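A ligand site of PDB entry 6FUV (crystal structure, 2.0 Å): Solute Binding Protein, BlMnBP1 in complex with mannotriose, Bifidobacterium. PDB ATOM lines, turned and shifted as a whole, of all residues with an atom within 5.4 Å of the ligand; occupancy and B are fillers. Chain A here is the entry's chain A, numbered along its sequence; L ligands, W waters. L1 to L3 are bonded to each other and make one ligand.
The side-chain amide oxygen of Gln 273 is in hydrogen-bond range of the side-chain amino group of Lys 253 (3.4 Å). NH2 of Arg 30 lies close to NE2 of Gln 273 (3.3 Å). OE1 of Glu 250 is in salt-bridge range of NZ of Lys 253, 2.7 Å away. OE1 of Gln 132 is in hydrogen-bond range of N of Trp 269 (2.8 Å). The side-chain carboxylate of Asp 32 is in salt-bridge range of the guanidinium group of Arg 30 (2.7 Å). The indole nitrogen of Trp 182 sits at hydrogen-bond distance from the side-chain carboxylate of Glu 180 (2.8 Å). The backbone NH of Gln 132 is in hydrogen-bond range of the backbone carbonyl oxygen of Ala 302.
O of Gly 29 touches C5 of LIG L1, 3.9 Å away. CD of Arg 30 touches O3 of LIG L1, at 3.6 Å. Thr 31 touches the ligand. CB of Asp 32 touches O1 of LIG L1 (3.5 Å). CB of Gln 132 touches O2 of LG3 L3, 3.9 Å away. NE1 of Trp 182 touches C6 of LIG L1, at 3.5 Å. CD2 of Tyr 305 touches O5 of LG2 L2, 3.7 Å away. Of the 20 residues printed, 15 come within 4 Å of the ligand. The nearest printed residue that does not touch the ligand is Ser 65 (4.3 Å).
The side-chain amide oxygen (OE1) of Gln 273 is in hydrogen-bond range of an oxygen (O2) of LIG L1 (2.6 Å). The side-chain carboxylate of Glu 250 sits at hydrogen-bond distance from an oxygen (O1) of LIG L1 (2.7 Å). The indole nitrogen (NE1) of Trp 249 lies within hydrogen-bond range of an oxygen (O2) of LIG L1 (2.9 Å). An oxygen (O2) of LIG L1 is in hydrogen-bond range of the side-chain amino group (NZ) of Lys 253, 2.9 Å away. O of Gly 303 lies within hydrogen-bond range of O2 of LG3 L3, 3.1 Å away. NE2 of Gln 189 lies within hydrogen-bond range of O1 of LG3 L3 (3.2 Å). The indole nitrogen (NE1) of Trp 269 sits at hydrogen-bond distance from an oxygen (O1) of LG3 L3. The side-chain amide oxygen (OD1) of Asn 304 lies within hydrogen-bond range of an oxygen (O5) of LG2 L2, at 3.4 Å.
Water W1 lies within hydrogen-bond range of OH of Tyr 305 (2.5 Å) and O2 of LG2 L2 (2.8 Å). Water W6 lies within hydrogen-bond range of an oxygen (O1) of LG3 L3 (2.9 Å), the side-chain amide oxygen (OE1) of Gln 189 (3.4 Å) and the indole nitrogen (NE1) of Trp 269 (3.4 Å). Water W7 lies within hydrogen-bond range of O1 of LG2 L2 (3.2 Å) and N of Tyr 67 (3.3 Å). Water W3 lies within hydrogen-bond range of the indole nitrogen of Trp 269 (3.1 Å), an oxygen (O1) of LG3 L3 (3.3 Å) and the side-chain amide oxygen of Gln 189 (3.4 Å). Water W8 bridges the backbone carbonyl oxygen (O) of Gly 29 (2.6 Å) and an oxygen (O6) of LIG L1 (3.4 Å).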
ATOM      1  N   GLY A  29       2.525 -24.355  -5.775  1.00  0.00           N
ATOM      2  CA  GLY A  29       1.283 -24.237  -6.518  1.00  0.00           C
ATOM      3  C   GLY A  29       1.081 -25.269  -7.604  1.00  0.00           C
ATOM      4  O   GLY A  29       0.093 -25.232  -8.343  1.00  0.00           O
ATOM      5  N   ARG A  30       2.002 -26.202  -7.749  1.00  0.00           N
ATOM      6  CA  ARG A  30       1.882 -27.232  -8.756  1.00  0.00           C
ATOM      7  C   ARG A  30       0.960 -28.338  -8.239  1.00  0.00           C
ATOM      8  O   ARG A  30       1.356 -29.444  -7.866  1.00  0.00           O
ATOM      9  CB  ARG A  30       3.247 -27.751  -9.127  1.00  0.00           C
ATOM     10  CG  ARG A  30       4.111 -26.791  -9.938  1.00  0.00           C
ATOM     11  CD  ARG A  30       3.456 -26.361 -11.207  1.00  0.00           C
ATOM     12  NE  ARG A  30       3.080 -27.440 -12.085  1.00  0.00           N
ATOM     13  CZ  ARG A  30       3.831 -27.948 -13.059  1.00  0.00           C
ATOM     14  NH1 ARG A  30       5.058 -27.536 -13.242  1.00  0.00           N
ATOM     15  NH2 ARG A  30       3.361 -28.910 -13.839  1.00  0.00           N
ATOM     16  N   THR A  31      -0.324 -27.999  -8.195  1.00  0.00           N
ATOM     17  CA  THR A  31      -1.293 -28.970  -7.710  1.00  0.00           C
ATOM     18  C   THR A  31      -1.337 -30.171  -8.634  1.00  0.00           C
ATOM     19  O   THR A  31      -1.444 -31.309  -8.181  1.00  0.00           O
ATOM     20  CB  THR A  31      -2.682 -28.357  -7.555  1.00  0.00           C
ATOM     21  OG1 THR A  31      -3.076 -27.783  -8.795  1.00  0.00           O
ATOM     22  CG2 THR A  31      -2.719 -27.299  -6.478  1.00  0.00           C
ATOM     23  N   ASP A  32      -1.180 -29.926  -9.941  1.00  0.00           N
ATOM     24  CA  ASP A  32      -1.106 -31.012 -10.903  1.00  0.00           C
ATOM     25  C   ASP A  32      -0.029 -32.023 -10.525  1.00  0.00           C
ATOM     26  O   ASP A  32      -0.273 -33.231 -10.581  1.00  0.00           O
ATOM     27  CB  ASP A  32      -0.872 -30.458 -12.325  1.00  0.00           C
ATOM     28  CG  ASP A  32       0.345 -29.559 -12.481  1.00  0.00           C
ATOM     29  OD1 ASP A  32       0.951 -29.078 -11.485  1.00  0.00           O
ATOM     30  OD2 ASP A  32       0.693 -29.306 -13.685  1.00  0.00           O
ATOM     31  N   SER A  65      -4.307 -24.508  -4.740  1.00  0.00           N
ATOM     32  CA  SER A  65      -4.801 -23.618  -5.776  1.00  0.00           C
ATOM     33  C   SER A  65      -4.896 -22.196  -5.182  1.00  0.00           C
ATOM     34  O   SER A  65      -4.774 -21.975  -3.978  1.00  0.00           O
ATOM     35  CB  SER A  65      -6.134 -24.133  -6.330  1.00  0.00           C
ATOM     36  OG  SER A  65      -7.143 -23.986  -5.405  1.00  0.00           O
ATOM     37  N   ASN A  66      -5.101 -21.238  -6.059  1.00  0.00           N
ATOM     38  CA  ASN A  66      -4.925 -19.823  -5.721  1.00  0.00           C
ATOM     39  C   ASN A  66      -3.688 -19.650  -4.827  1.00  0.00           C
ATOM     40  O   ASN A  66      -3.753 -19.088  -3.726  1.00  0.00           O
ATOM     41  CB  ASN A  66      -6.157 -19.238  -5.063  1.00  0.00           C
ATOM     42  CG  ASN A  66      -6.089 -17.688  -4.933  1.00  0.00           C
ATOM     43  OD1 ASN A  66      -5.396 -17.005  -5.699  1.00  0.00           O
ATOM     44  ND2 ASN A  66      -6.815 -17.145  -3.947  1.00  0.00           N
ATOM     45  N   TYR A  67      -2.564 -20.145  -5.342  1.00  0.00           N
ATOM     46  CA  TYR A  67      -1.330 -20.137  -4.566  1.00  0.00           C
ATOM     47  C   TYR A  67      -0.914 -18.728  -4.198  1.00  0.00           C
ATOM     48  O   TYR A  67      -0.313 -18.512  -3.156  1.00  0.00           O
ATOM     49  CB  TYR A  67      -0.194 -20.815  -5.346  1.00  0.00           C
ATOM     50  CG  TYR A  67       1.084 -20.849  -4.557  1.00  0.00           C
ATOM     51  CD1 TYR A  67       1.273 -21.780  -3.562  1.00  0.00           C
ATOM     52  CD2 TYR A  67       2.087 -19.911  -4.768  1.00  0.00           C
ATOM     53  CE1 TYR A  67       2.424 -21.805  -2.837  1.00  0.00           C
ATOM     54  CE2 TYR A  67       3.175 -19.910  -4.017  1.00  0.00           C
ATOM     55  CZ  TYR A  67       3.359 -20.871  -3.043  1.00  0.00           C
ATOM     56  OH  TYR A  67       4.470 -20.906  -2.283  1.00  0.00           O
ATOM     57  N   GLN A 132      12.242 -18.616 -17.154  1.00  0.00           N
ATOM     58  CA  GLN A 132      10.987 -18.526 -17.888  1.00  0.00           C
ATOM     59  C   GLN A 132      11.012 -17.368 -18.865  1.00  0.00           C
ATOM     60  O   GLN A 132      11.679 -16.331 -18.649  1.00  0.00           O
ATOM     61  CB  GLN A 132       9.785 -18.404 -16.929  1.00  0.00           C
ATOM     62  CG  GLN A 132       9.318 -19.752 -16.390  1.00  0.00           C
ATOM     63  CD  GLN A 132       8.810 -20.690 -17.456  1.00  0.00           C
ATOM     64  OE1 GLN A 132       8.012 -20.330 -18.271  1.00  0.00           O
ATOM     65  NE2 GLN A 132       9.282 -21.924 -17.436  1.00  0.00           N
ATOM     66  N   GLU A 180      -9.256 -17.021 -13.771  1.00  0.00           N
ATOM     67  CA  GLU A 180      -8.037 -17.195 -12.997  1.00  0.00           C
ATOM     68  C   GLU A 180      -7.332 -15.851 -12.946  1.00  0.00           C
ATOM     69  O   GLU A 180      -6.879 -15.342 -13.954  1.00  0.00           O
ATOM     70  CB  GLU A 180      -7.139 -18.276 -13.607  1.00  0.00           C
ATOM     71  CG  GLU A 180      -7.734 -19.635 -13.605  1.00  0.00           C
ATOM     72  CD  GLU A 180      -7.776 -20.297 -12.242  1.00  0.00           C
ATOM     73  OE1 GLU A 180      -6.970 -19.949 -11.391  1.00  0.00           O
ATOM     74  OE2 GLU A 180      -8.639 -21.187 -12.018  1.00  0.00           O
ATOM     75  N   TRP A 182      -4.407 -15.086 -11.636  1.00  0.00           N
ATOM     76  CA  TRP A 182      -3.011 -15.233 -12.055  1.00  0.00           C
ATOM     77  C   TRP A 182      -2.903 -15.279 -13.575  1.00  0.00           C
ATOM     78  O   TRP A 182      -1.967 -14.733 -14.164  1.00  0.00           O
ATOM     79  CB  TRP A 182      -2.357 -16.488 -11.407  1.00  0.00           C
ATOM     80  CG  TRP A 182      -2.954 -17.802 -11.755  1.00  0.00           C
ATOM     81  CD1 TRP A 182      -3.838 -18.512 -11.028  1.00  0.00           C
ATOM     82  CD2 TRP A 182      -2.769 -18.518 -12.966  1.00  0.00           C
ATOM     83  NE1 TRP A 182      -4.170 -19.648 -11.670  1.00  0.00           N
ATOM     84  CE2 TRP A 182      -3.537 -19.669 -12.887  1.00  0.00           C
ATOM     85  CE3 TRP A 182      -2.006 -18.302 -14.114  1.00  0.00           C
ATOM     86  CZ2 TRP A 182      -3.615 -20.587 -13.934  1.00  0.00           C
ATOM     87  CZ3 TRP A 182      -2.056 -19.225 -15.116  1.00  0.00           C
ATOM     88  CH2 TRP A 182      -2.859 -20.347 -15.030  1.00  0.00           C
ATOM     89  N   GLN A 189       3.517  -9.659 -17.807  1.00  0.00           N
ATOM     90  CA  GLN A 189       4.840 -10.248 -18.035  1.00  0.00           C
ATOM     91  C   GLN A 189       5.427  -9.828 -19.363  1.00  0.00           C
ATOM     92  O   GLN A 189       6.625  -9.996 -19.583  1.00  0.00           O
ATOM     93  CB  GLN A 189       4.725 -11.792 -17.942  1.00  0.00           C
ATOM     94  CG  GLN A 189       4.247 -12.280 -16.649  1.00  0.00           C
ATOM     95  CD  GLN A 189       4.167 -13.760 -16.531  1.00  0.00           C
ATOM     96  OE1 GLN A 189       4.537 -14.503 -17.416  1.00  0.00           O
ATOM     97  NE2 GLN A 189       3.734 -14.199 -15.389  1.00  0.00           N
ATOM     98  N   TRP A 249      -9.503 -23.322 -16.078  1.00  0.00           N
ATOM     99  CA  TRP A 249      -8.099 -23.520 -16.384  1.00  0.00           C
ATOM    100  C   TRP A 249      -7.784 -24.960 -16.715  1.00  0.00           C
ATOM    101  O   TRP A 249      -7.178 -25.228 -17.745  1.00  0.00           O
ATOM    102  CB  TRP A 249      -7.252 -23.072 -15.194  1.00  0.00           C
ATOM    103  CG  TRP A 249      -5.848 -23.522 -15.197  1.00  0.00           C
ATOM    104  CD1 TRP A 249      -5.275 -24.300 -14.287  1.00  0.00           C
ATOM    105  CD2 TRP A 249      -4.833 -23.260 -16.193  1.00  0.00           C
ATOM    106  NE1 TRP A 249      -3.985 -24.533 -14.603  1.00  0.00           N
ATOM    107  CE2 TRP A 249      -3.685 -23.918 -15.783  1.00  0.00           C
ATOM    108  CE3 TRP A 249      -4.799 -22.541 -17.390  1.00  0.00           C
ATOM    109  CZ2 TRP A 249      -2.489 -23.859 -16.521  1.00  0.00           C
ATOM    110  CZ3 TRP A 249      -3.644 -22.451 -18.077  1.00  0.00           C
ATOM    111  CH2 TRP A 249      -2.507 -23.126 -17.658  1.00  0.00           C
ATOM    112  N   GLU A 250      -8.115 -25.891 -15.816  1.00  0.00           N
ATOM    113  CA  GLU A 250      -7.669 -27.268 -16.032  1.00  0.00           C
ATOM    114  C   GLU A 250      -8.234 -27.837 -17.339  1.00  0.00           C
ATOM    115  O   GLU A 250      -7.538 -28.573 -18.065  1.00  0.00           O
ATOM    116  CB  GLU A 250      -8.083 -28.174 -14.889  1.00  0.00           C
ATOM    117  CG  GLU A 250      -7.453 -27.877 -13.549  1.00  0.00           C
ATOM    118  CD  GLU A 250      -5.935 -27.994 -13.536  1.00  0.00           C
ATOM    119  OE1 GLU A 250      -5.375 -28.669 -14.402  1.00  0.00           O
ATOM    120  OE2 GLU A 250      -5.352 -27.446 -12.591  1.00  0.00           O
ATOM    121  N   LYS A 253      -6.445 -26.749 -20.785  1.00  0.00           N
ATOM    122  CA  LYS A 253      -5.286 -27.519 -21.227  1.00  0.00           C
ATOM    123  C   LYS A 253      -5.702 -28.570 -22.247  1.00  0.00           C
ATOM    124  O   LYS A 253      -5.081 -28.730 -23.299  1.00  0.00           O
ATOM    125  CB  LYS A 253      -4.608 -28.172 -20.024  1.00  0.00           C
ATOM    126  CG  LYS A 253      -4.047 -27.226 -18.959  1.00  0.00           C
ATOM    127  CD  LYS A 253      -3.581 -28.033 -17.737  1.00  0.00           C
ATOM    128  CE  LYS A 253      -3.386 -27.172 -16.539  1.00  0.00           C
ATOM    129  NZ  LYS A 253      -2.946 -27.891 -15.339  1.00  0.00           N
ATOM    130  N   TRP A 269       6.302 -22.256 -19.351  1.00  0.00           N
ATOM    131  CA  TRP A 269       5.998 -23.306 -18.388  1.00  0.00           C
ATOM    132  C   TRP A 269       4.708 -23.991 -18.760  1.00  0.00           C
ATOM    133  O   TRP A 269       4.527 -25.155 -18.439  1.00  0.00           O
ATOM    134  CB  TRP A 269       5.907 -22.701 -16.995  1.00  0.00           C
ATOM    135  CG  TRP A 269       4.829 -21.691 -16.922  1.00  0.00           C
ATOM    136  CD1 TRP A 269       4.940 -20.364 -17.113  1.00  0.00           C
ATOM    137  CD2 TRP A 269       3.440 -21.950 -16.693  1.00  0.00           C
ATOM    138  NE1 TRP A 269       3.717 -19.749 -16.980  1.00  0.00           N
ATOM    139  CE2 TRP A 269       2.768 -20.700 -16.742  1.00  0.00           C
ATOM    140  CE3 TRP A 269       2.696 -23.104 -16.438  1.00  0.00           C
ATOM    141  CZ2 TRP A 269       1.379 -20.579 -16.534  1.00  0.00           C
ATOM    142  CZ3 TRP A 269       1.334 -22.970 -16.263  1.00  0.00           C
ATOM    143  CH2 TRP A 269       0.681 -21.724 -16.322  1.00  0.00           C
ATOM    144  N   GLN A 273       2.567 -28.708 -20.064  1.00  0.00           N
ATOM    145  CA  GLN A 273       1.343 -29.090 -19.371  1.00  0.00           C
ATOM    146  C   GLN A 273       0.231 -29.328 -20.389  1.00  0.00           C
ATOM    147  O   GLN A 273      -0.630 -30.187 -20.193  1.00  0.00           O
ATOM    148  CB  GLN A 273       0.894 -27.997 -18.371  1.00  0.00           C
ATOM    149  CG  GLN A 273       1.865 -27.703 -17.227  1.00  0.00           C
ATOM    150  CD  GLN A 273       1.312 -26.798 -16.142  1.00  0.00           C
ATOM    151  OE1 GLN A 273       0.128 -26.615 -15.989  1.00  0.00           O
ATOM    152  NE2 GLN A 273       2.203 -26.266 -15.352  1.00  0.00           N
ATOM    153  N   ALA A 302      13.093 -14.192 -17.125  1.00  0.00           N
ATOM    154  CA  ALA A 302      12.871 -13.967 -15.703  1.00  0.00           C
ATOM    155  C   ALA A 302      12.527 -15.301 -15.070  1.00  0.00           C
ATOM    156  O   ALA A 302      12.165 -16.267 -15.739  1.00  0.00           O
ATOM    157  CB  ALA A 302      11.777 -12.928 -15.425  1.00  0.00           C
ATOM    158  N   GLY A 303      12.701 -15.369 -13.766  1.00  0.00           N
ATOM    159  CA  GLY A 303      12.457 -16.624 -13.091  1.00  0.00           C
ATOM    160  C   GLY A 303      11.006 -17.079 -13.114  1.00  0.00           C
ATOM    161  O   GLY A 303      10.058 -16.277 -13.183  1.00  0.00           O
ATOM    162  N   ASN A 304      10.873 -18.383 -13.077  1.00  0.00           N
ATOM    163  CA  ASN A 304       9.616 -18.999 -12.620  1.00  0.00           C
ATOM    164  C   ASN A 304       9.482 -18.649 -11.124  1.00  0.00           C
ATOM    165  O   ASN A 304      10.272 -17.851 -10.598  1.00  0.00           O
ATOM    166  CB  ASN A 304       9.680 -20.490 -12.879  1.00  0.00           C
ATOM    167  CG  ASN A 304       8.311 -21.111 -12.999  1.00  0.00           C
ATOM    168  OD1 ASN A 304       7.335 -20.550 -12.566  1.00  0.00           O
ATOM    169  ND2 ASN A 304       8.235 -22.267 -13.622  1.00  0.00           N
ATOM    170  N   TYR A 305       8.545 -19.234 -10.407  1.00  0.00           N
ATOM    171  CA  TYR A 305       8.472 -19.085  -8.955  1.00  0.00           C
ATOM    172  C   TYR A 305       9.809 -19.517  -8.372  1.00  0.00           C
ATOM    173  O   TYR A 305      10.399 -20.501  -8.855  1.00  0.00           O
ATOM    174  CB  TYR A 305       7.330 -19.920  -8.344  1.00  0.00           C
ATOM    175  CG  TYR A 305       5.994 -19.175  -8.153  1.00  0.00           C
ATOM    176  CD1 TYR A 305       5.859 -18.209  -7.210  1.00  0.00           C
ATOM    177  CD2 TYR A 305       4.888 -19.511  -8.879  1.00  0.00           C
ATOM    178  CE1 TYR A 305       4.662 -17.527  -7.023  1.00  0.00           C
ATOM    179  CE2 TYR A 305       3.688 -18.870  -8.699  1.00  0.00           C
ATOM    180  CZ  TYR A 305       3.586 -17.860  -7.755  1.00  0.00           C
ATOM    181  OH  TYR A 305       2.401 -17.223  -7.563  1.00  0.00           O
HETATM  182  C1  LIG L   1      -1.981 -26.429 -11.856  1.00  0.00           C
HETATM  183  C2  LIG L   1      -0.874 -26.118 -12.861  1.00  0.00           C
HETATM  184  C3  LIG L   1      -0.066 -24.902 -12.350  1.00  0.00           C
HETATM  185  C4  LIG L   1      -1.048 -23.717 -12.146  1.00  0.00           C
HETATM  186  C5  LIG L   1      -2.222 -24.128 -11.254  1.00  0.00           C
HETATM  187  C6  LIG L   1      -3.292 -23.015 -11.108  1.00  0.00           C
HETATM  188  O1  LIG L   1      -2.685 -27.484 -12.338  1.00  0.00           O
HETATM  189  O2  LIG L   1      -1.431 -25.742 -14.127  1.00  0.00           O
HETATM  190  O3  LIG L   1       1.011 -24.632 -13.221  1.00  0.00           O
HETATM  191  O4  LIG L   1      -0.451 -22.602 -11.478  1.00  0.00           O
HETATM  192  O5  LIG L   1      -2.846 -25.326 -11.789  1.00  0.00           O
HETATM  193  O6  LIG L   1      -4.215 -23.380 -10.079  1.00  0.00           O
HETATM  194  C1  LG2 L   2       0.261 -21.782 -12.367  1.00  0.00           C
HETATM  195  C2  LG2 L   2       0.118 -20.368 -11.744  1.00  0.00           C
HETATM  196  C3  LG2 L   2       1.008 -19.443 -12.445  1.00  0.00           C
HETATM  197  C4  LG2 L   2       2.457 -19.958 -12.601  1.00  0.00           C
HETATM  198  C5  LG2 L   2       2.479 -21.383 -13.146  1.00  0.00           C
HETATM  199  C6  LG2 L   2       3.864 -22.021 -13.042  1.00  0.00           C
HETATM  200  O1  LG2 L   2       0.531 -20.358 -10.401  1.00  0.00           O
HETATM  201  O2  LG2 L   2       0.966 -18.206 -11.757  1.00  0.00           O
HETATM  202  O3  LG2 L   2       3.152 -19.083 -13.536  1.00  0.00           O
HETATM  203  O4  LG2 L   2       1.572 -22.198 -12.317  1.00  0.00           O
HETATM  204  O5  LG2 L   2       4.319 -21.938 -11.648  1.00  0.00           O
HETATM  205  C1  LG3 L   3       4.241 -18.355 -12.941  1.00  0.00           C
HETATM  206  C2  LG3 L   3       5.252 -18.012 -14.028  1.00  0.00           C
HETATM  207  C3  LG3 L   3       6.376 -17.108 -13.479  1.00  0.00           C
HETATM  208  C4  LG3 L   3       5.725 -15.939 -12.679  1.00  0.00           C
HETATM  209  C5  LG3 L   3       4.781 -16.485 -11.644  1.00  0.00           C
HETATM  210  C6  LG3 L   3       4.142 -15.389 -10.798  1.00  0.00           C
HETATM  211  O1  LG3 L   3       4.542 -17.286 -15.059  1.00  0.00           O
HETATM  212  O2  LG3 L   3       7.283 -16.605 -14.494  1.00  0.00           O
HETATM  213  O3  LG3 L   3       6.689 -15.180 -12.041  1.00  0.00           O
HETATM  214  O4  LG3 L   3       3.749 -17.197 -12.313  1.00  0.00           O
HETATM  215  O5  LG3 L   3       3.264 -14.639 -11.605  1.00  0.00           O
HETATM  216  O   HOH W   1       0.447 -17.300  -9.170  1.00  0.00           O
HETATM  217  O   HOH W   2       1.712 -17.280 -15.198  1.00  0.00           O
HETATM  218  O   HOH W   3       2.342 -17.065 -17.535  1.00  0.00           O
HETATM  219  O   HOH W   4       3.160 -12.044 -10.058  1.00  0.00           O
HETATM  220  O   HOH W   5       2.648 -22.406  -9.250  1.00  0.00           O
HETATM  221  O   HOH W   6       6.152 -17.441 -17.446  1.00  0.00           O
HETATM  222  O   HOH W   7      -1.993 -20.900  -8.545  1.00  0.00           O
HETATM  223  O   HOH W   8      -1.717 -23.491  -7.738  1.00  0.00           O
